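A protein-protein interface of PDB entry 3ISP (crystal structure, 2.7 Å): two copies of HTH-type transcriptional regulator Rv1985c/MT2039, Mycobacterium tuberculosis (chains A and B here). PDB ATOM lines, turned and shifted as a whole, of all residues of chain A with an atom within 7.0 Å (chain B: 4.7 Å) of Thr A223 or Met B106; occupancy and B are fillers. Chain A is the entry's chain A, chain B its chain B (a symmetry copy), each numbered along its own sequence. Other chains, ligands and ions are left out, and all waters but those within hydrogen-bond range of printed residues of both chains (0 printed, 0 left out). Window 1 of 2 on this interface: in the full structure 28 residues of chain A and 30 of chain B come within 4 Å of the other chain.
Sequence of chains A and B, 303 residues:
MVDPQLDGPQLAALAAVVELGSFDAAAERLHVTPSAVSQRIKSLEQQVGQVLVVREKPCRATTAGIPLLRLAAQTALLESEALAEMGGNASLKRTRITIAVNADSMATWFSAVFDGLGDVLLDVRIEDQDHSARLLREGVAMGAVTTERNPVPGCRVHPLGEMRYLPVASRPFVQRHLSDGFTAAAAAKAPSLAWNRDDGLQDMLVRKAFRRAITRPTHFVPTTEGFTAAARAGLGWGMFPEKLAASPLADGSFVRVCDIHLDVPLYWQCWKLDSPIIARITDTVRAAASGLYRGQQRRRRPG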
ATOM      1  N   ALA A 103      22.633 -19.456 -20.956  1.00  0.00           N
ATOM      2  CA  ALA A 103      21.754 -20.431 -20.301  1.00  0.00           C
ATOM      3  C   ALA A 103      20.972 -21.299 -21.274  1.00  0.00           C
ATOM      4  O   ALA A 103      20.914 -22.509 -21.126  1.00  0.00           O
ATOM      5  CB  ALA A 103      20.794 -19.715 -19.354  1.00  0.00           C
ATOM      6  N   TRP A 195      13.556 -13.697 -17.671  1.00  0.00           N
ATOM      7  CA  TRP A 195      14.622 -14.109 -16.775  1.00  0.00           C
ATOM      8  C   TRP A 195      14.994 -12.989 -15.827  1.00  0.00           C
ATOM      9  O   TRP A 195      15.383 -13.235 -14.684  1.00  0.00           O
ATOM     10  CB  TRP A 195      15.851 -14.557 -17.570  1.00  0.00           C
ATOM     11  CG  TRP A 195      15.710 -15.941 -18.065  1.00  0.00           C
ATOM     12  CD1 TRP A 195      14.701 -16.437 -18.852  1.00  0.00           C
ATOM     13  CD2 TRP A 195      16.589 -17.031 -17.802  1.00  0.00           C
ATOM     14  NE1 TRP A 195      14.904 -17.779 -19.087  1.00  0.00           N
ATOM     15  CE2 TRP A 195      16.057 -18.167 -18.453  1.00  0.00           C
ATOM     16  CE3 TRP A 195      17.769 -17.162 -17.074  1.00  0.00           C
ATOM     17  CZ2 TRP A 195      16.673 -19.407 -18.405  1.00  0.00           C
ATOM     18  CZ3 TRP A 195      18.377 -18.404 -17.022  1.00  0.00           C
ATOM     19  CH2 TRP A 195      17.828 -19.510 -17.689  1.00  0.00           C
ATOM     20  N   VAL A 221      11.691 -14.871 -13.451  1.00  0.00           N
ATOM     21  CA  VAL A 221      12.095 -16.171 -12.952  1.00  0.00           C
ATOM     22  C   VAL A 221      13.251 -16.712 -13.777  1.00  0.00           C
ATOM     23  O   VAL A 221      13.091 -17.041 -14.953  1.00  0.00           O
ATOM     24  CB  VAL A 221      10.951 -17.190 -12.980  1.00  0.00           C
ATOM     25  CG1 VAL A 221      11.298 -18.354 -12.081  1.00  0.00           C
ATOM     26  CG2 VAL A 221       9.650 -16.552 -12.536  1.00  0.00           C
ATOM     27  N   PRO A 222      14.425 -16.816 -13.148  1.00  0.00           N
ATOM     28  CA  PRO A 222      15.650 -17.222 -13.824  1.00  0.00           C
ATOM     29  C   PRO A 222      15.837 -18.732 -13.762  1.00  0.00           C
ATOM     30  O   PRO A 222      15.105 -19.413 -13.038  1.00  0.00           O
ATOM     31  CB  PRO A 222      16.733 -16.539 -12.998  1.00  0.00           C
ATOM     32  CG  PRO A 222      16.004 -15.849 -11.826  1.00  0.00           C
ATOM     33  CD  PRO A 222      14.676 -16.477 -11.743  1.00  0.00           C
ATOM     34  N   THR A 223      16.820 -19.218 -14.524  1.00  0.00           N
ATOM     35  CA  THR A 223      17.189 -20.634 -14.647  1.00  0.00           C
ATOM     36  C   THR A 223      16.229 -21.409 -15.537  1.00  0.00           C
ATOM     37  O   THR A 223      15.104 -20.983 -15.775  1.00  0.00           O
ATOM     38  CB  THR A 223      17.390 -21.351 -13.276  1.00  0.00           C
ATOM     39  OG1 THR A 223      16.129 -21.727 -12.721  1.00  0.00           O
ATOM     40  CG2 THR A 223      18.128 -20.455 -12.307  1.00  0.00           C
ATOM     41  N   THR A 224      16.692 -22.545 -16.032  1.00  0.00           N
ATOM     42  CA  THR A 224      15.880 -23.360 -16.922  1.00  0.00           C
ATOM     43  C   THR A 224      14.705 -23.967 -16.163  1.00  0.00           C
ATOM     44  O   THR A 224      13.556 -23.889 -16.616  1.00  0.00           O
ATOM     45  CB  THR A 224      16.718 -24.478 -17.595  1.00  0.00           C
ATOM     46  OG1 THR A 224      17.715 -23.880 -18.430  1.00  0.00           O
ATOM     47  CG2 THR A 224      15.840 -25.400 -18.437  1.00  0.00           C
ATOM     48  N   GLU A 225      14.985 -24.570 -15.008  1.00  0.00           N
ATOM     49  CA  GLU A 225      13.914 -25.179 -14.224  1.00  0.00           C
ATOM     50  C   GLU A 225      12.974 -24.099 -13.695  1.00  0.00           C
ATOM     51  O   GLU A 225      11.757 -24.252 -13.734  1.00  0.00           O
ATOM     52  CB  GLU A 225      14.480 -26.039 -13.084  1.00  0.00           C
ATOM     53  CG  GLU A 225      15.899 -25.641 -12.629  1.00  0.00           C
ATOM     54  CD  GLU A 225      17.006 -26.229 -13.507  1.00  0.00           C
ATOM     55  OE1 GLU A 225      16.782 -27.301 -14.120  1.00  0.00           O
ATOM     56  OE2 GLU A 225      18.104 -25.623 -13.576  1.00  0.00           O
ATOM     57  N   GLY A 226      13.554 -23.000 -13.224  1.00  0.00           N
ATOM     58  CA  GLY A 226      12.789 -21.888 -12.702  1.00  0.00           C
ATOM     59  C   GLY A 226      11.852 -21.290 -13.727  1.00  0.00           C
ATOM     60  O   GLY A 226      10.660 -21.125 -13.457  1.00  0.00           O
ATOM     61  N   PHE A 227      12.392 -20.957 -14.899  1.00  0.00           N
ATOM     62  CA  PHE A 227      11.615 -20.360 -15.981  1.00  0.00           C
ATOM     63  C   PHE A 227      10.628 -21.377 -16.485  1.00  0.00           C
ATOM     64  O   PHE A 227       9.504 -21.028 -16.842  1.00  0.00           O
ATOM     65  CB  PHE A 227      12.527 -19.956 -17.133  1.00  0.00           C
ATOM     66  CG  PHE A 227      11.921 -18.964 -18.090  1.00  0.00           C
ATOM     67  CD1 PHE A 227      11.791 -17.630 -17.738  1.00  0.00           C
ATOM     68  CD2 PHE A 227      11.539 -19.351 -19.359  1.00  0.00           C
ATOM     69  CE1 PHE A 227      11.257 -16.704 -18.617  1.00  0.00           C
ATOM     70  CE2 PHE A 227      11.011 -18.428 -20.251  1.00  0.00           C
ATOM     71  CZ  PHE A 227      10.868 -17.102 -19.873  1.00  0.00           C
ATOM     72  N   THR A 228      11.041 -22.641 -16.507  1.00  0.00           N
ATOM     73  CA  THR A 228      10.165 -23.690 -17.022  1.00  0.00           C
ATOM     74  C   THR A 228       8.970 -23.981 -16.095  1.00  0.00           C
ATOM     75  O   THR A 228       7.840 -24.151 -16.572  1.00  0.00           O
ATOM     76  CB  THR A 228      10.933 -24.987 -17.383  1.00  0.00           C
ATOM     77  OG1 THR A 228      11.793 -24.731 -18.499  1.00  0.00           O
ATOM     78  CG2 THR A 228       9.967 -26.097 -17.769  1.00  0.00           C
ATOM     79  N   ALA A 229       9.211 -24.029 -14.785  1.00  0.00           N
ATOM     80  CA  ALA A 229       8.123 -24.239 -13.830  1.00  0.00           C
ATOM     81  C   ALA A 229       7.126 -23.081 -13.878  1.00  0.00           C
ATOM     82  O   ALA A 229       5.922 -23.291 -13.905  1.00  0.00           O
ATOM     83  CB  ALA A 229       8.660 -24.437 -12.418  1.00  0.00           C
ATOM     84  N   VAL B 101      16.357 -17.732  -3.728  1.00  0.00           N
ATOM     85  CA  VAL B 101      16.359 -19.191  -3.568  1.00  0.00           C
ATOM     86  C   VAL B 101      17.706 -19.764  -4.006  1.00  0.00           C
ATOM     87  O   VAL B 101      18.314 -19.281  -4.961  1.00  0.00           O
ATOM     88  CB  VAL B 101      15.250 -19.874  -4.418  1.00  0.00           C
ATOM     89  CG1 VAL B 101      15.069 -21.313  -4.007  1.00  0.00           C
ATOM     90  CG2 VAL B 101      13.925 -19.137  -4.289  1.00  0.00           C
ATOM     91  N   ASN B 102      18.187 -20.786  -3.310  1.00  0.00           N
ATOM     92  CA  ASN B 102      19.407 -21.448  -3.736  1.00  0.00           C
ATOM     93  C   ASN B 102      19.108 -22.375  -4.917  1.00  0.00           C
ATOM     94  O   ASN B 102      17.999 -22.887  -5.056  1.00  0.00           O
ATOM     95  CB  ASN B 102      20.053 -22.213  -2.583  1.00  0.00           C
ATOM     96  CG  ASN B 102      19.178 -23.335  -2.065  1.00  0.00           C
ATOM     97  OD1 ASN B 102      18.083 -23.104  -1.548  1.00  0.00           O
ATOM     98  ND2 ASN B 102      19.662 -24.562  -2.191  1.00  0.00           N
ATOM     99  N   ALA B 103      20.098 -22.598  -5.768  1.00  0.00           N
ATOM    100  CA  ALA B 103      19.864 -23.270  -7.037  1.00  0.00           C
ATOM    101  C   ALA B 103      19.234 -24.653  -6.910  1.00  0.00           C
ATOM    102  O   ALA B 103      18.349 -24.996  -7.686  1.00  0.00           O
ATOM    103  CB  ALA B 103      21.145 -23.332  -7.838  1.00  0.00           C
ATOM    104  N   ASP B 104      19.683 -25.445  -5.943  1.00  0.00           N
ATOM    105  CA  ASP B 104      19.219 -26.818  -5.818  1.00  0.00           C
ATOM    106  C   ASP B 104      17.787 -26.867  -5.349  1.00  0.00           C
ATOM    107  O   ASP B 104      17.128 -27.899  -5.449  1.00  0.00           O
ATOM    108  CB  ASP B 104      20.069 -27.582  -4.820  1.00  0.00           C
ATOM    109  CG  ASP B 104      21.467 -27.775  -5.288  1.00  0.00           C
ATOM    110  OD1 ASP B 104      21.651 -28.048  -6.491  1.00  0.00           O
ATOM    111  OD2 ASP B 104      22.385 -27.659  -4.452  1.00  0.00           O
ATOM    112  N   SER B 105      17.311 -25.762  -4.793  1.00  0.00           N
ATOM    113  CA  SER B 105      15.927 -25.688  -4.348  1.00  0.00           C
ATOM    114  C   SER B 105      15.041 -25.324  -5.525  1.00  0.00           C
ATOM    115  O   SER B 105      13.976 -25.915  -5.707  1.00  0.00           O
ATOM    116  CB  SER B 105      15.771 -24.667  -3.221  1.00  0.00           C
ATOM    117  OG  SER B 105      16.295 -25.180  -2.016  1.00  0.00           O
ATOM    118  N   MET B 106      15.477 -24.352  -6.322  1.00  0.00           N
ATOM    119  CA  MET B 106      14.730 -23.997  -7.516  1.00  0.00           C
ATOM    120  C   MET B 106      14.703 -25.176  -8.460  1.00  0.00           C
ATOM    121  O   MET B 106      13.800 -25.302  -9.278  1.00  0.00           O
ATOM    122  CB  MET B 106      15.349 -22.802  -8.233  1.00  0.00           C
ATOM    123  CG  MET B 106      14.563 -22.384  -9.457  1.00  0.00           C
ATOM    124  SD  MET B 106      12.871 -21.946  -9.025  1.00  0.00           S
ATOM    125  CE  MET B 106      13.124 -20.232  -8.669  1.00  0.00           C
ATOM    126  N   ALA B 107      15.700 -26.043  -8.350  1.00  0.00           N
ATOM    127  CA  ALA B 107      15.838 -27.151  -9.283  1.00  0.00           C
ATOM    128  C   ALA B 107      15.023 -28.335  -8.831  1.00  0.00           C
ATOM    129  O   ALA B 107      14.962 -29.354  -9.512  1.00  0.00           O
ATOM    130  CB  ALA B 107      17.290 -27.549  -9.411  1.00  0.00           C
ATOM    131  N   THR B 108      14.369 -28.181  -7.689  1.00  0.00           N
ATOM    132  CA  THR B 108      13.887 -29.335  -6.954  1.00  0.00           C
ATOM    133  C   THR B 108      12.482 -29.137  -6.367  1.00  0.00           C
ATOM    134  O   THR B 108      11.507 -29.540  -6.970  1.00  0.00           O
ATOM    135  CB  THR B 108      14.957 -29.766  -5.902  1.00  0.00           C
ATOM    136  OG1 THR B 108      15.244 -31.160  -6.031  1.00  0.00           O
ATOM    137  CG2 THR B 108      14.538 -29.453  -4.486  1.00  0.00           C
ATOM    138  N   PHE B 110      11.142 -26.014  -4.841  1.00  0.00           N
ATOM    139  CA  PHE B 110      10.620 -24.670  -4.708  1.00  0.00           C
ATOM    140  C   PHE B 110       9.538 -24.353  -5.709  1.00  0.00           C
ATOM    141  O   PHE B 110       8.704 -23.494  -5.451  1.00  0.00           O
ATOM    142  CB  PHE B 110      11.740 -23.640  -4.834  1.00  0.00           C
ATOM    143  CG  PHE B 110      11.310 -22.243  -4.516  1.00  0.00           C
ATOM    144  CD1 PHE B 110      10.984 -21.362  -5.520  1.00  0.00           C
ATOM    145  CD2 PHE B 110      11.234 -21.814  -3.213  1.00  0.00           C
ATOM    146  CE1 PHE B 110      10.590 -20.095  -5.226  1.00  0.00           C
ATOM    147  CE2 PHE B 110      10.850 -20.543  -2.924  1.00  0.00           C
ATOM    148  CZ  PHE B 110      10.519 -19.686  -3.927  1.00  0.00           C
ATOM    149  N   PHE B 114       4.838 -22.017  -7.141  1.00  0.00           N
ATOM    150  CA  PHE B 114       4.245 -21.275  -8.242  1.00  0.00           C
ATOM    151  C   PHE B 114       2.750 -21.525  -8.356  1.00  0.00           C
ATOM    152  O   PHE B 114       2.011 -20.656  -8.822  1.00  0.00           O
ATOM    153  CB  PHE B 114       4.937 -21.580  -9.574  1.00  0.00           C
ATOM    154  CG  PHE B 114       6.358 -21.091  -9.652  1.00  0.00           C
ATOM    155  CD1 PHE B 114       6.748 -19.942  -8.979  1.00  0.00           C
ATOM    156  CD2 PHE B 114       7.297 -21.767 -10.417  1.00  0.00           C
ATOM    157  CE1 PHE B 114       8.045 -19.484  -9.052  1.00  0.00           C
ATOM    158  CE2 PHE B 114       8.592 -21.308 -10.498  1.00  0.00           C
ATOM    159  CZ  PHE B 114       8.971 -20.166  -9.807  1.00  0.00           C
ATOM    160  N   VAL B 124      12.094 -13.520  -8.744  1.00  0.00           N
ATOM    161  CA  VAL B 124      12.911 -14.599  -8.196  1.00  0.00           C
ATOM    162  C   VAL B 124      14.393 -14.509  -8.531  1.00  0.00           C
ATOM    163  O   VAL B 124      14.794 -14.394  -9.694  1.00  0.00           O
ATOM    164  CB  VAL B 124      12.378 -15.967  -8.611  1.00  0.00           C
ATOM    165  CG1 VAL B 124      13.270 -17.048  -8.085  1.00  0.00           C
ATOM    166  CG2 VAL B 124      10.988 -16.145  -8.077  1.00  0.00           C
ATOM    167  N   ILE B 126      18.232 -16.306  -7.943  1.00  0.00           N
ATOM    168  CA  ILE B 126      18.953 -17.523  -7.621  1.00  0.00           C
ATOM    169  C   ILE B 126      20.309 -17.164  -7.032  1.00  0.00           C
ATOM    170  O   ILE B 126      21.216 -16.717  -7.735  1.00  0.00           O
ATOM    171  CB  ILE B 126      19.107 -18.439  -8.833  1.00  0.00           C
ATOM    172  CG1 ILE B 126      17.732 -18.763  -9.411  1.00  0.00           C
ATOM    173  CG2 ILE B 126      19.800 -19.724  -8.425  1.00  0.00           C
ATOM    174  CD1 ILE B 126      16.716 -19.165  -8.357  1.00  0.00           C
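OG1 of Thr A223 sits at hydrogen-bond distance from N of Gly A226, 2.9 Å away.
Among the printed residues, pairs that only touch across the chains: Pro A222 with Val B124, Thr A223 with Ile B126, Ala A229 with Phe B114, Gly A226 with Phe B114, Glu A225 with Ala B107, Gly A226 with Met B106, Thr A223 with Met B106, Val A221 with Phe B114 and Glu A225 with Met B106.
Of the printed residues of chain B, Pro A222 touches Val B124 (2.9 Å).
Thr A223 touches just these residues of chain B: Met B106 and Ile B126.
Met B106 touches just these residues of chain A: Thr A223, Glu A225 and Gly A226.
Printed residues of chain A within 4 Å of Ala B107: Glu A225 (3.7 Å).
Of the printed residues of chain A, Val B124 touches Pro A222.
The nearest printed residue of chain B that does not touch Val A221 is Met B106 (4.3 Å).
Hydrophobic or aromatic side chains of chain B within 4 Å of the printed part of chain A: Met B106, Ala B107, Phe B114, Val B124 and Ile B126.
Hydrophobic or aromatic side chains of chain A that line the printed part of chain B: Val A221, Pro A222 and Ala A229.
Among the printed residues, 9 pairs touch across the chains.
Position printed for both chains: 103.
Of the 9 pairs that touch across the chains among the printed residues, none has its exchanged pair printed and touching as well.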
